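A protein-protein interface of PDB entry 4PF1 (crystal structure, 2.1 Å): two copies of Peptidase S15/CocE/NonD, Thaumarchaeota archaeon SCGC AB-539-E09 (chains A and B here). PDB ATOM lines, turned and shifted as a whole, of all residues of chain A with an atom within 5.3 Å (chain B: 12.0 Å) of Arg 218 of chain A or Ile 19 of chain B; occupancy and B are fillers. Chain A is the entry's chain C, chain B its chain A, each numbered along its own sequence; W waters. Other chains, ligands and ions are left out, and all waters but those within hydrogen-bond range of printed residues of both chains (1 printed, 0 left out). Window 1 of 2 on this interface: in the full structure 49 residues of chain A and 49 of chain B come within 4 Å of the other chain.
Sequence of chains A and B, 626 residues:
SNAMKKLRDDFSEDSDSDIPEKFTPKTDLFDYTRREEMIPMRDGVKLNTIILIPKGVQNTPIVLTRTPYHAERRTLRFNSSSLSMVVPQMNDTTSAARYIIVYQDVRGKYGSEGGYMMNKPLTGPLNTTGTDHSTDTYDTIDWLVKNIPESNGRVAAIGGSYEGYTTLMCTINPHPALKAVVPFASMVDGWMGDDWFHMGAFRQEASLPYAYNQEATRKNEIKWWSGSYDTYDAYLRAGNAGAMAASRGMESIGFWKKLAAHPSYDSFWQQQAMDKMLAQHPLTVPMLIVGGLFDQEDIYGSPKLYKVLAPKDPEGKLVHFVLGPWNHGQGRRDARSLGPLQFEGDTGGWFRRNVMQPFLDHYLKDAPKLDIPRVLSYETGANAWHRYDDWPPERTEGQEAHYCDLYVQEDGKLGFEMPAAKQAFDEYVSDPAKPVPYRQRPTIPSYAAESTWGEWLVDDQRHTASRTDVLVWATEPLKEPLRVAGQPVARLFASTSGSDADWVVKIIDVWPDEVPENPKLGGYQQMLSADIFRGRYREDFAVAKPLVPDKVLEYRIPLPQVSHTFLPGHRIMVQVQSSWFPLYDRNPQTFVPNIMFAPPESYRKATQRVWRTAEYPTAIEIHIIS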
ATOM      1  N   GLY A 108     -10.240  15.069  -5.663  1.00  0.00           N
ATOM      2  CA  GLY A 108     -11.539  15.479  -5.144  1.00  0.00           C
ATOM      3  C   GLY A 108     -12.408  16.353  -6.029  1.00  0.00           C
ATOM      4  O   GLY A 108     -13.509  16.727  -5.612  1.00  0.00           O
ATOM      5  N   LYS A 109     -11.947  16.691  -7.250  1.00  0.00           N
ATOM      6  CA  LYS A 109     -12.748  17.529  -8.149  1.00  0.00           C
ATOM      7  C   LYS A 109     -13.143  16.805  -9.436  1.00  0.00           C
ATOM      8  O   LYS A 109     -12.329  16.096 -10.033  1.00  0.00           O
ATOM      9  CB  LYS A 109     -12.026  18.851  -8.496  1.00  0.00           C
ATOM     10  CG  LYS A 109     -12.076  19.936  -7.399  1.00  0.00           C
ATOM     11  CD  LYS A 109     -13.499  20.274  -6.861  1.00  0.00           C
ATOM     12  CE  LYS A 109     -14.350  21.060  -7.832  1.00  0.00           C
ATOM     13  NZ  LYS A 109     -15.777  21.084  -7.408  1.00  0.00           N
ATOM     14  N   TYR A 110     -14.408  17.017  -9.861  1.00  0.00           N
ATOM     15  CA  TYR A 110     -15.026  16.523 -11.096  1.00  0.00           C
ATOM     16  C   TYR A 110     -14.858  14.994 -11.321  1.00  0.00           C
ATOM     17  O   TYR A 110     -15.560  14.214 -10.683  1.00  0.00           O
ATOM     18  CB  TYR A 110     -14.536  17.335 -12.308  1.00  0.00           C
ATOM     19  CG  TYR A 110     -15.096  18.743 -12.333  1.00  0.00           C
ATOM     20  CD1 TYR A 110     -16.368  18.999 -12.840  1.00  0.00           C
ATOM     21  CD2 TYR A 110     -14.386  19.807 -11.786  1.00  0.00           C
ATOM     22  CE1 TYR A 110     -16.905  20.284 -12.830  1.00  0.00           C
ATOM     23  CE2 TYR A 110     -14.908  21.101 -11.783  1.00  0.00           C
ATOM     24  CZ  TYR A 110     -16.168  21.335 -12.311  1.00  0.00           C
ATOM     25  OH  TYR A 110     -16.676  22.612 -12.347  1.00  0.00           O
ATOM     26  N   SER A 112     -12.061  13.128 -10.865  1.00  0.00           N
ATOM     27  CA  SER A 112     -11.083  12.517  -9.966  1.00  0.00           C
ATOM     28  C   SER A 112     -11.704  12.053  -8.660  1.00  0.00           C
ATOM     29  O   SER A 112     -12.609  12.706  -8.137  1.00  0.00           O
ATOM     30  CB  SER A 112      -9.953  13.493  -9.668  1.00  0.00           C
ATOM     31  OG  SER A 112      -9.111  13.646 -10.795  1.00  0.00           O
ATOM     32  N   GLU A 113     -11.177  10.941  -8.109  1.00  0.00           N
ATOM     33  CA  GLU A 113     -11.612  10.365  -6.832  1.00  0.00           C
ATOM     34  C   GLU A 113     -10.966  11.107  -5.660  1.00  0.00           C
ATOM     35  O   GLU A 113     -10.124  11.985  -5.869  1.00  0.00           O
ATOM     36  CB  GLU A 113     -11.243   8.867  -6.759  1.00  0.00           C
ATOM     37  CG  GLU A 113     -11.984   7.977  -7.743  1.00  0.00           C
ATOM     38  CD  GLU A 113     -11.398   6.589  -7.929  1.00  0.00           C
ATOM     39  OE1 GLU A 113     -10.438   6.235  -7.205  1.00  0.00           O
ATOM     40  OE2 GLU A 113     -11.899   5.855  -8.810  1.00  0.00           O
ATOM     41  N   GLY A 114     -11.334  10.714  -4.442  1.00  0.00           N
ATOM     42  CA  GLY A 114     -10.786  11.272  -3.213  1.00  0.00           C
ATOM     43  C   GLY A 114     -11.520  12.491  -2.698  1.00  0.00           C
ATOM     44  O   GLY A 114     -12.500  12.940  -3.300  1.00  0.00           O
ATOM     45  N   GLY A 115     -11.049  13.000  -1.565  1.00  0.00           N
ATOM     46  CA  GLY A 115     -11.599  14.191  -0.932  1.00  0.00           C
ATOM     47  C   GLY A 115     -10.965  15.453  -1.472  1.00  0.00           C
ATOM     48  O   GLY A 115      -9.861  15.406  -2.026  1.00  0.00           O
ATOM     49  N   TYR A 116     -11.656  16.595  -1.329  1.00  0.00           N
ATOM     50  CA  TYR A 116     -11.130  17.862  -1.824  1.00  0.00           C
ATOM     51  C   TYR A 116     -10.822  18.827  -0.685  1.00  0.00           C
ATOM     52  O   TYR A 116     -11.663  19.064   0.184  1.00  0.00           O
ATOM     53  CB  TYR A 116     -12.089  18.512  -2.840  1.00  0.00           C
ATOM     54  CG  TYR A 116     -11.596  19.848  -3.363  1.00  0.00           C
ATOM     55  CD1 TYR A 116     -10.483  19.925  -4.198  1.00  0.00           C
ATOM     56  CD2 TYR A 116     -12.222  21.036  -2.998  1.00  0.00           C
ATOM     57  CE1 TYR A 116     -10.001  21.153  -4.648  1.00  0.00           C
ATOM     58  CE2 TYR A 116     -11.753  22.268  -3.451  1.00  0.00           C
ATOM     59  CZ  TYR A 116     -10.644  22.323  -4.278  1.00  0.00           C
ATOM     60  OH  TYR A 116     -10.177  23.532  -4.725  1.00  0.00           O
ATOM     61  N   GLN A 214     -17.484  25.619  -6.020  1.00  0.00           N
ATOM     62  CA  GLN A 214     -16.376  24.667  -6.020  1.00  0.00           C
ATOM     63  C   GLN A 214     -16.461  23.596  -4.916  1.00  0.00           C
ATOM     64  O   GLN A 214     -15.779  22.575  -5.034  1.00  0.00           O
ATOM     65  CB  GLN A 214     -15.031  25.415  -5.900  1.00  0.00           C
ATOM     66  CG  GLN A 214     -14.678  26.283  -7.117  1.00  0.00           C
ATOM     67  CD  GLN A 214     -14.389  25.470  -8.359  1.00  0.00           C
ATOM     68  OE1 GLN A 214     -15.087  25.572  -9.372  1.00  0.00           O
ATOM     69  NE2 GLN A 214     -13.350  24.647  -8.308  1.00  0.00           N
ATOM     70  N   GLU A 215     -17.244  23.821  -3.837  1.00  0.00           N
ATOM     71  CA  GLU A 215     -17.239  22.857  -2.720  1.00  0.00           C
ATOM     72  C   GLU A 215     -18.614  22.268  -2.312  1.00  0.00           C
ATOM     73  O   GLU A 215     -18.642  21.385  -1.448  1.00  0.00           O
ATOM     74  CB  GLU A 215     -16.558  23.461  -1.486  1.00  0.00           C
ATOM     75  CG  GLU A 215     -15.100  23.821  -1.723  1.00  0.00           C
ATOM     76  CD  GLU A 215     -14.264  23.998  -0.476  1.00  0.00           C
ATOM     77  OE1 GLU A 215     -14.843  24.250   0.606  1.00  0.00           O
ATOM     78  OE2 GLU A 215     -13.025  23.841  -0.573  1.00  0.00           O
ATOM     79  N   ALA A 216     -19.734  22.721  -2.913  1.00  0.00           N
ATOM     80  CA  ALA A 216     -21.048  22.140  -2.587  1.00  0.00           C
ATOM     81  C   ALA A 216     -21.130  20.700  -3.100  1.00  0.00           C
ATOM     82  O   ALA A 216     -21.658  19.827  -2.410  1.00  0.00           O
ATOM     83  CB  ALA A 216     -22.172  22.977  -3.182  1.00  0.00           C
ATOM     84  N   THR A 217     -20.578  20.460  -4.306  1.00  0.00           N
ATOM     85  CA  THR A 217     -20.517  19.147  -4.964  1.00  0.00           C
ATOM     86  C   THR A 217     -19.151  18.957  -5.636  1.00  0.00           C
ATOM     87  O   THR A 217     -18.446  19.940  -5.900  1.00  0.00           O
ATOM     88  CB  THR A 217     -21.643  19.000  -6.007  1.00  0.00           C
ATOM     89  OG1 THR A 217     -21.628  20.128  -6.879  1.00  0.00           O
ATOM     90  CG2 THR A 217     -23.020  18.823  -5.380  1.00  0.00           C
ATOM     91  N   ARG A 218     -18.799  17.692  -5.946  1.00  0.00           N
ATOM     92  CA  ARG A 218     -17.553  17.325  -6.626  1.00  0.00           C
ATOM     93  C   ARG A 218     -17.515  17.885  -8.057  1.00  0.00           C
ATOM     94  O   ARG A 218     -16.477  18.390  -8.501  1.00  0.00           O
ATOM     95  CB  ARG A 218     -17.415  15.783  -6.662  1.00  0.00           C
ATOM     96  CG  ARG A 218     -16.075  15.267  -7.204  1.00  0.00           C
ATOM     97  CD  ARG A 218     -16.063  13.753  -7.384  1.00  0.00           C
ATOM     98  NE  ARG A 218     -16.214  13.039  -6.112  1.00  0.00           N
ATOM     99  CZ  ARG A 218     -15.201  12.678  -5.330  1.00  0.00           C
ATOM    100  NH1 ARG A 218     -13.950  12.952  -5.682  1.00  0.00           N
ATOM    101  NH2 ARG A 218     -15.430  12.041  -4.189  1.00  0.00           N
ATOM    102  N   LYS A 219     -18.649  17.794  -8.769  1.00  0.00           N
ATOM    103  CA  LYS A 219     -18.747  18.165 -10.175  1.00  0.00           C
ATOM    104  C   LYS A 219     -19.508  19.490 -10.417  1.00  0.00           C
ATOM    105  O   LYS A 219     -20.024  19.688 -11.521  1.00  0.00           O
ATOM    106  CB  LYS A 219     -19.414  17.021 -10.964  1.00  0.00           C
ATOM    107  CG  LYS A 219     -18.718  15.675 -10.797  1.00  0.00           C
ATOM    108  CD  LYS A 219     -19.496  14.551 -11.446  1.00  0.00           C
ATOM    109  CE  LYS A 219     -18.783  13.231 -11.285  1.00  0.00           C
ATOM    110  NZ  LYS A 219     -19.449  12.148 -12.052  1.00  0.00           N
ATOM    111  N   ASN A 220     -19.520  20.416  -9.419  1.00  0.00           N
ATOM    112  CA  ASN A 220     -20.190  21.735  -9.518  1.00  0.00           C
ATOM    113  C   ASN A 220     -21.643  21.602 -10.053  1.00  0.00           C
ATOM    114  O   ASN A 220     -22.037  22.298 -10.994  1.00  0.00           O
ATOM    115  CB  ASN A 220     -19.377  22.704 -10.402  1.00  0.00           C
ATOM    116  CG  ASN A 220     -18.140  23.280  -9.754  1.00  0.00           C
ATOM    117  OD1 ASN A 220     -17.407  22.608  -9.013  1.00  0.00           O
ATOM    118  ND2 ASN A 220     -17.847  24.530 -10.077  1.00  0.00           N
ATOM    119  N   GLU A 221     -22.408  20.676  -9.466  1.00  0.00           N
ATOM    120  CA  GLU A 221     -23.787  20.404  -9.869  1.00  0.00           C
ATOM    121  C   GLU A 221     -24.755  21.379  -9.187  1.00  0.00           C
ATOM    122  O   GLU A 221     -25.870  21.576  -9.673  1.00  0.00           O
ATOM    123  CB  GLU A 221     -24.156  18.946  -9.553  1.00  0.00           C
ATOM    124  CG  GLU A 221     -23.326  17.944 -10.338  1.00  0.00           C
ATOM    125  CD  GLU A 221     -23.159  16.596  -9.668  1.00  0.00           C
ATOM    126  OE1 GLU A 221     -24.034  15.723  -9.865  1.00  0.00           O
ATOM    127  OE2 GLU A 221     -22.138  16.402  -8.967  1.00  0.00           O
ATOM    128  N   GLY A 254     -16.453  23.301   3.860  1.00  0.00           N
ATOM    129  CA  GLY A 254     -15.135  23.246   4.484  1.00  0.00           C
ATOM    130  C   GLY A 254     -14.299  24.507   4.422  1.00  0.00           C
ATOM    131  O   GLY A 254     -13.712  24.894   5.436  1.00  0.00           O
ATOM    132  N   PHE B  11     -15.260  18.484  12.534  1.00  0.00           N
ATOM    133  CA  PHE B  11     -14.542  18.732  11.286  1.00  0.00           C
ATOM    134  C   PHE B  11     -13.056  18.973  11.562  1.00  0.00           C
ATOM    135  O   PHE B  11     -12.709  19.834  12.377  1.00  0.00           O
ATOM    136  CB  PHE B  11     -15.159  19.930  10.525  1.00  0.00           C
ATOM    137  CG  PHE B  11     -14.448  20.327   9.246  1.00  0.00           C
ATOM    138  CD1 PHE B  11     -14.651  19.618   8.068  1.00  0.00           C
ATOM    139  CD2 PHE B  11     -13.606  21.432   9.214  1.00  0.00           C
ATOM    140  CE1 PHE B  11     -14.003  19.992   6.886  1.00  0.00           C
ATOM    141  CE2 PHE B  11     -12.959  21.806   8.031  1.00  0.00           C
ATOM    142  CZ  PHE B  11     -13.162  21.083   6.876  1.00  0.00           C
ATOM    143  N   SER B  12     -12.183  18.206  10.884  1.00  0.00           N
ATOM    144  CA  SER B  12     -10.735  18.349  11.016  1.00  0.00           C
ATOM    145  C   SER B  12     -10.171  19.022   9.766  1.00  0.00           C
ATOM    146  O   SER B  12     -10.273  18.478   8.665  1.00  0.00           O
ATOM    147  CB  SER B  12     -10.071  16.998  11.269  1.00  0.00           C
ATOM    148  OG  SER B  12     -10.368  16.064  10.243  1.00  0.00           O
ATOM    149  N   GLU B  13      -9.610  20.230   9.941  1.00  0.00           N
ATOM    150  CA  GLU B  13      -9.053  21.057   8.857  1.00  0.00           C
ATOM    151  C   GLU B  13      -7.826  20.408   8.183  1.00  0.00           C
ATOM    152  O   GLU B  13      -7.488  20.769   7.051  1.00  0.00           O
ATOM    153  CB  GLU B  13      -8.664  22.446   9.394  1.00  0.00           C
ATOM    154  CG  GLU B  13      -9.811  23.208  10.043  1.00  0.00           C
ATOM    155  CD  GLU B  13      -9.444  24.548  10.656  1.00  0.00           C
ATOM    156  OE1 GLU B  13      -8.243  24.779  10.930  1.00  0.00           O
ATOM    157  OE2 GLU B  13     -10.369  25.361  10.890  1.00  0.00           O
ATOM    158  N   ASP B  14      -7.165  19.464   8.882  1.00  0.00           N
ATOM    159  CA  ASP B  14      -5.949  18.793   8.421  1.00  0.00           C
ATOM    160  C   ASP B  14      -6.208  17.505   7.602  1.00  0.00           C
ATOM    161  O   ASP B  14      -5.250  16.942   7.064  1.00  0.00           O
ATOM    162  CB  ASP B  14      -5.035  18.465   9.625  1.00  0.00           C
ATOM    163  CG  ASP B  14      -5.758  17.925  10.854  1.00  0.00           C
ATOM    164  OD1 ASP B  14      -6.593  17.004  10.701  1.00  0.00           O
ATOM    165  OD2 ASP B  14      -5.468  18.407  11.970  1.00  0.00           O
ATOM    166  N   SER B  15      -7.471  17.027   7.509  1.00  0.00           N
ATOM    167  CA  SER B  15      -7.732  15.768   6.800  1.00  0.00           C
ATOM    168  C   SER B  15      -9.096  15.692   6.107  1.00  0.00           C
ATOM    169  O   SER B  15      -9.178  15.134   5.010  1.00  0.00           O
ATOM    170  CB  SER B  15      -7.597  14.584   7.755  1.00  0.00           C
ATOM    171  OG  SER B  15      -8.333  14.792   8.950  1.00  0.00           O
ATOM    172  N   ASP B  16     -10.167  16.186   6.757  1.00  0.00           N
ATOM    173  CA  ASP B  16     -11.528  16.081   6.221  1.00  0.00           C
ATOM    174  C   ASP B  16     -11.716  16.812   4.904  1.00  0.00           C
ATOM    175  O   ASP B  16     -11.146  17.889   4.692  1.00  0.00           O
ATOM    176  CB  ASP B  16     -12.565  16.581   7.237  1.00  0.00           C
ATOM    177  CG  ASP B  16     -12.879  15.589   8.340  1.00  0.00           C
ATOM    178  OD1 ASP B  16     -12.437  14.421   8.235  1.00  0.00           O
ATOM    179  OD2 ASP B  16     -13.571  15.977   9.303  1.00  0.00           O
ATOM    180  N   SER B  17     -12.521  16.208   4.013  1.00  0.00           N
ATOM    181  CA  SER B  17     -12.875  16.783   2.725  1.00  0.00           C
ATOM    182  C   SER B  17     -13.772  17.986   2.950  1.00  0.00           C
ATOM    183  O   SER B  17     -14.664  17.941   3.803  1.00  0.00           O
ATOM    184  CB  SER B  17     -13.576  15.748   1.850  1.00  0.00           C
ATOM    185  OG  SER B  17     -13.892  16.280   0.573  1.00  0.00           O
ATOM    186  N   ASP B  18     -13.513  19.075   2.217  1.00  0.00           N
ATOM    187  CA  ASP B  18     -14.280  20.309   2.327  1.00  0.00           C
ATOM    188  C   ASP B  18     -15.682  20.145   1.737  1.00  0.00           C
ATOM    189  O   ASP B  18     -16.600  20.866   2.131  1.00  0.00           O
ATOM    190  CB  ASP B  18     -13.541  21.457   1.628  1.00  0.00           C
ATOM    191  CG  ASP B  18     -12.321  21.994   2.365  1.00  0.00           C
ATOM    192  OD1 ASP B  18     -12.177  21.700   3.573  1.00  0.00           O
ATOM    193  OD2 ASP B  18     -11.542  22.747   1.749  1.00  0.00           O
ATOM    194  N   ILE B  19     -15.839  19.195   0.798  1.00  0.00           N
ATOM    195  CA  ILE B  19     -17.111  18.917   0.142  1.00  0.00           C
ATOM    196  C   ILE B  19     -17.958  17.991   1.030  1.00  0.00           C
ATOM    197  O   ILE B  19     -17.561  16.845   1.265  1.00  0.00           O
ATOM    198  CB  ILE B  19     -16.901  18.322  -1.289  1.00  0.00           C
ATOM    199  CG1 ILE B  19     -16.081  19.294  -2.189  1.00  0.00           C
ATOM    200  CG2 ILE B  19     -18.253  17.944  -1.938  1.00  0.00           C
ATOM    201  CD1 ILE B  19     -15.677  18.752  -3.591  1.00  0.00           C
ATOM    202  N   PRO B  20     -19.137  18.456   1.522  1.00  0.00           N
ATOM    203  CA  PRO B  20     -19.994  17.563   2.328  1.00  0.00           C
ATOM    204  C   PRO B  20     -20.549  16.418   1.479  1.00  0.00           C
ATOM    205  O   PRO B  20     -20.674  16.568   0.262  1.00  0.00           O
ATOM    206  CB  PRO B  20     -21.107  18.492   2.824  1.00  0.00           C
ATOM    207  CG  PRO B  20     -21.175  19.575   1.814  1.00  0.00           C
ATOM    208  CD  PRO B  20     -19.765  19.781   1.332  1.00  0.00           C
ATOM    209  N   GLU B  21     -20.847  15.264   2.115  1.00  0.00           N
ATOM    210  CA  GLU B  21     -21.371  14.072   1.433  1.00  0.00           C
ATOM    211  C   GLU B  21     -22.668  14.397   0.679  1.00  0.00           C
ATOM    212  O   GLU B  21     -22.808  14.031  -0.491  1.00  0.00           O
ATOM    213  CB  GLU B  21     -21.594  12.926   2.439  1.00  0.00           C
ATOM    214  CG  GLU B  21     -21.723  11.545   1.804  1.00  0.00           C
ATOM    215  CD  GLU B  21     -20.513  11.039   1.035  1.00  0.00           C
ATOM    216  OE1 GLU B  21     -20.713  10.410  -0.030  1.00  0.00           O
ATOM    217  OE2 GLU B  21     -19.369  11.266   1.493  1.00  0.00           O
ATOM    218  N   LYS B  22     -23.586  15.123   1.335  1.00  0.00           N
ATOM    219  CA  LYS B  22     -24.850  15.537   0.738  1.00  0.00           C
ATOM    220  C   LYS B  22     -25.128  16.996   1.092  1.00  0.00           C
ATOM    221  O   LYS B  22     -25.230  17.340   2.273  1.00  0.00           O
ATOM    222  CB  LYS B  22     -26.001  14.623   1.207  1.00  0.00           C
ATOM    223  CG  LYS B  22     -27.327  14.876   0.493  1.00  0.00           C
ATOM    224  CD  LYS B  22     -28.496  14.246   1.239  1.00  0.00           C
ATOM    225  CE  LYS B  22     -29.828  14.670   0.671  1.00  0.00           C
ATOM    226  NZ  LYS B  22     -30.962  14.159   1.486  1.00  0.00           N
ATOM    227  N   PHE B  23     -25.217  17.854   0.072  1.00  0.00           N
ATOM    228  CA  PHE B  23     -25.517  19.267   0.260  1.00  0.00           C
ATOM    229  C   PHE B  23     -26.896  19.579  -0.296  1.00  0.00           C
ATOM    230  O   PHE B  23     -27.214  19.178  -1.418  1.00  0.00           O
ATOM    231  CB  PHE B  23     -24.447  20.161  -0.405  1.00  0.00           C
ATOM    232  CG  PHE B  23     -24.622  21.638  -0.123  1.00  0.00           C
ATOM    233  CD1 PHE B  23     -24.119  22.204   1.042  1.00  0.00           C
ATOM    234  CD2 PHE B  23     -25.292  22.461  -1.023  1.00  0.00           C
ATOM    235  CE1 PHE B  23     -24.290  23.565   1.307  1.00  0.00           C
ATOM    236  CE2 PHE B  23     -25.469  23.821  -0.753  1.00  0.00           C
ATOM    237  CZ  PHE B  23     -24.966  24.365   0.409  1.00  0.00           C
ATOM    238  N   THR B  24     -27.719  20.282   0.493  1.00  0.00           N
ATOM    239  CA  THR B  24     -29.058  20.699   0.077  1.00  0.00           C
ATOM    240  C   THR B  24     -29.115  22.230   0.119  1.00  0.00           C
ATOM    241  O   THR B  24     -28.887  22.816   1.182  1.00  0.00           O
ATOM    242  CB  THR B  24     -30.159  20.047   0.950  1.00  0.00           C
ATOM    243  OG1 THR B  24     -29.989  20.448   2.308  1.00  0.00           O
ATOM    244  CG2 THR B  24     -30.178  18.523   0.846  1.00  0.00           C
HETATM  245  O   HOH W   1     -21.911  17.153  -2.040  1.00  0.00           O
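OD2 of Asp 18 of chain B lies close to OE2 of Glu 215 of chain A (3.0 Å). The backbone carbonyl oxygen of Asp 18 of chain B lies within hydrogen-bond range of the backbone NH of Gly 254 of chain A (3.0 Å). N of Asp 18 of chain B is in hydrogen-bond range of O of Tyr 116 of chain A. OG of Ser 17 of chain B sits at hydrogen-bond distance from N of Tyr 116 of chain A.
O of Ser 112 of chain A sits at hydrogen-bond distance from NH1 of Arg 218 of chain A. The backbone NH (N) of Glu 221 of chain A sits at hydrogen-bond distance from the side-chain hydroxyl (OG1) of Thr 217 of chain A (2.8 Å). The guanidinium group (NH1) of Arg 218 of chain A sits at hydrogen-bond distance from the backbone carbonyl oxygen (O) of Gly 114 of chain A. The side-chain hydroxyl of Thr 217 of chain A sits at hydrogen-bond distance from the backbone NH of Asn 220 of chain A (3.3 Å). The side-chain amino group (NZ) of Lys 109 of chain A is in hydrogen-bond range of the backbone carbonyl oxygen (O) of Thr 217 of chain A (3.3 Å). The backbone carbonyl oxygen of Glu 113 of chain A is in hydrogen-bond range of the backbone NH of Gly 108 of chain A (3.1 Å).
Gly 108 of chain A touches Ile 19 of chain B. OG of Ser 17 of chain B touches CA of Gly 115 of chain A, at 3.4 Å. Ile 19 of chain B touches Tyr 116 of chain A (CD1 to CB, 3.7 Å). Glu 215 of chain A touches Ile 19 of chain B. Pro 20 of chain B touches Glu 215 of chain A (CD to O, 3.4 Å). Ala 216 of chain A touches Ile 19 of chain B (O to CG2, 3.9 Å). O of Ala 216 of chain A touches CB of Phe 23 of chain B, 3.5 Å away. Ile 19 of chain B touches Thr 217 of chain A (CD1 to O, 3.8 Å). CD1 of Ile 19 of chain B touches CA of Arg 218 of chain A, 3.8 Å away. Gly 254 of chain A touches Phe 11 of chain B (CA to CZ, 3.8 Å).
Arg 218 of chain A touches just one residue of chain B: Ile 19. Printed residues of chain A within 4 Å of Ile 19 of chain B: Gly 108 (3.6 Å), Tyr 116 (3.7 Å), Glu 215 (3.3 Å), Ala 216 (3.9 Å), Thr 217 (3.8 Å) and Arg 218 (3.8 Å). No residue of chain B comes within 4 Å of Lys 109 of chain A. No residue of chain B comes within 4 Å of Tyr 110 of chain A. Of chain B, only Ser 17 comes within 4 Å of Gly 115 of chain A. Of chain B, only Ser 17, Asp 18 and Ile 19 come within 4 Å of Tyr 116 of chain A. Glu 215 of chain A touches just these residues of chain B: Asp 18, Ile 19 and Pro 20. Of chain B, only Ile 19 and Phe 23 come within 4 Å of Ala 216 of chain A. Printed residues of chain B within 4 Å of Thr 217 of chain A: Ile 19. Asn 220 of chain A touches none of the printed residues of chain B. Gly 254 of chain A touches two residues of chain B. Of the printed residues of chain A, Pro 20 of chain B touches Glu 215. Of the printed residues of chain A, Asp 18 of chain B touches Tyr 116 (2.7 Å), Glu 215 (3.0 Å) and Gly 254 (3.0 Å). Of the printed residues of chain A, Ser 17 of chain B touches Gly 115 (3.4 Å) and Tyr 116 (3.0 Å). Glu 113 of chain A touches none of the printed residues of chain B. The nearest printed residue of chain B that does not touch Arg 218 of chain A is Ser 17 of chain B (6.6 Å). The nearest residue of chain A that does not touch Ile 19 of chain B is Gln 214 of chain A (4.1 Å).
Hydrophobic or aromatic side chains of chain B within 4 Å of the printed part of chain A: Phe 11, Ile 19, Pro 20 and Phe 23. Hydrophobic or aromatic side chains of chain A that line the printed part of chain B: Tyr 116 and Ala 216. Among the printed residues, 14 pairs touch across the chains. Among the printed residues, no Asp or Glu carboxylate lies within 4 Å of a Lys or Arg side-chain nitrogen of the other chain.
No position is printed for both chains.
Water W1 lies within hydrogen-bond range of O of Pro 20 of chain B (2.7 Å) and O of Ala 216 of chain A (2.7 Å).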
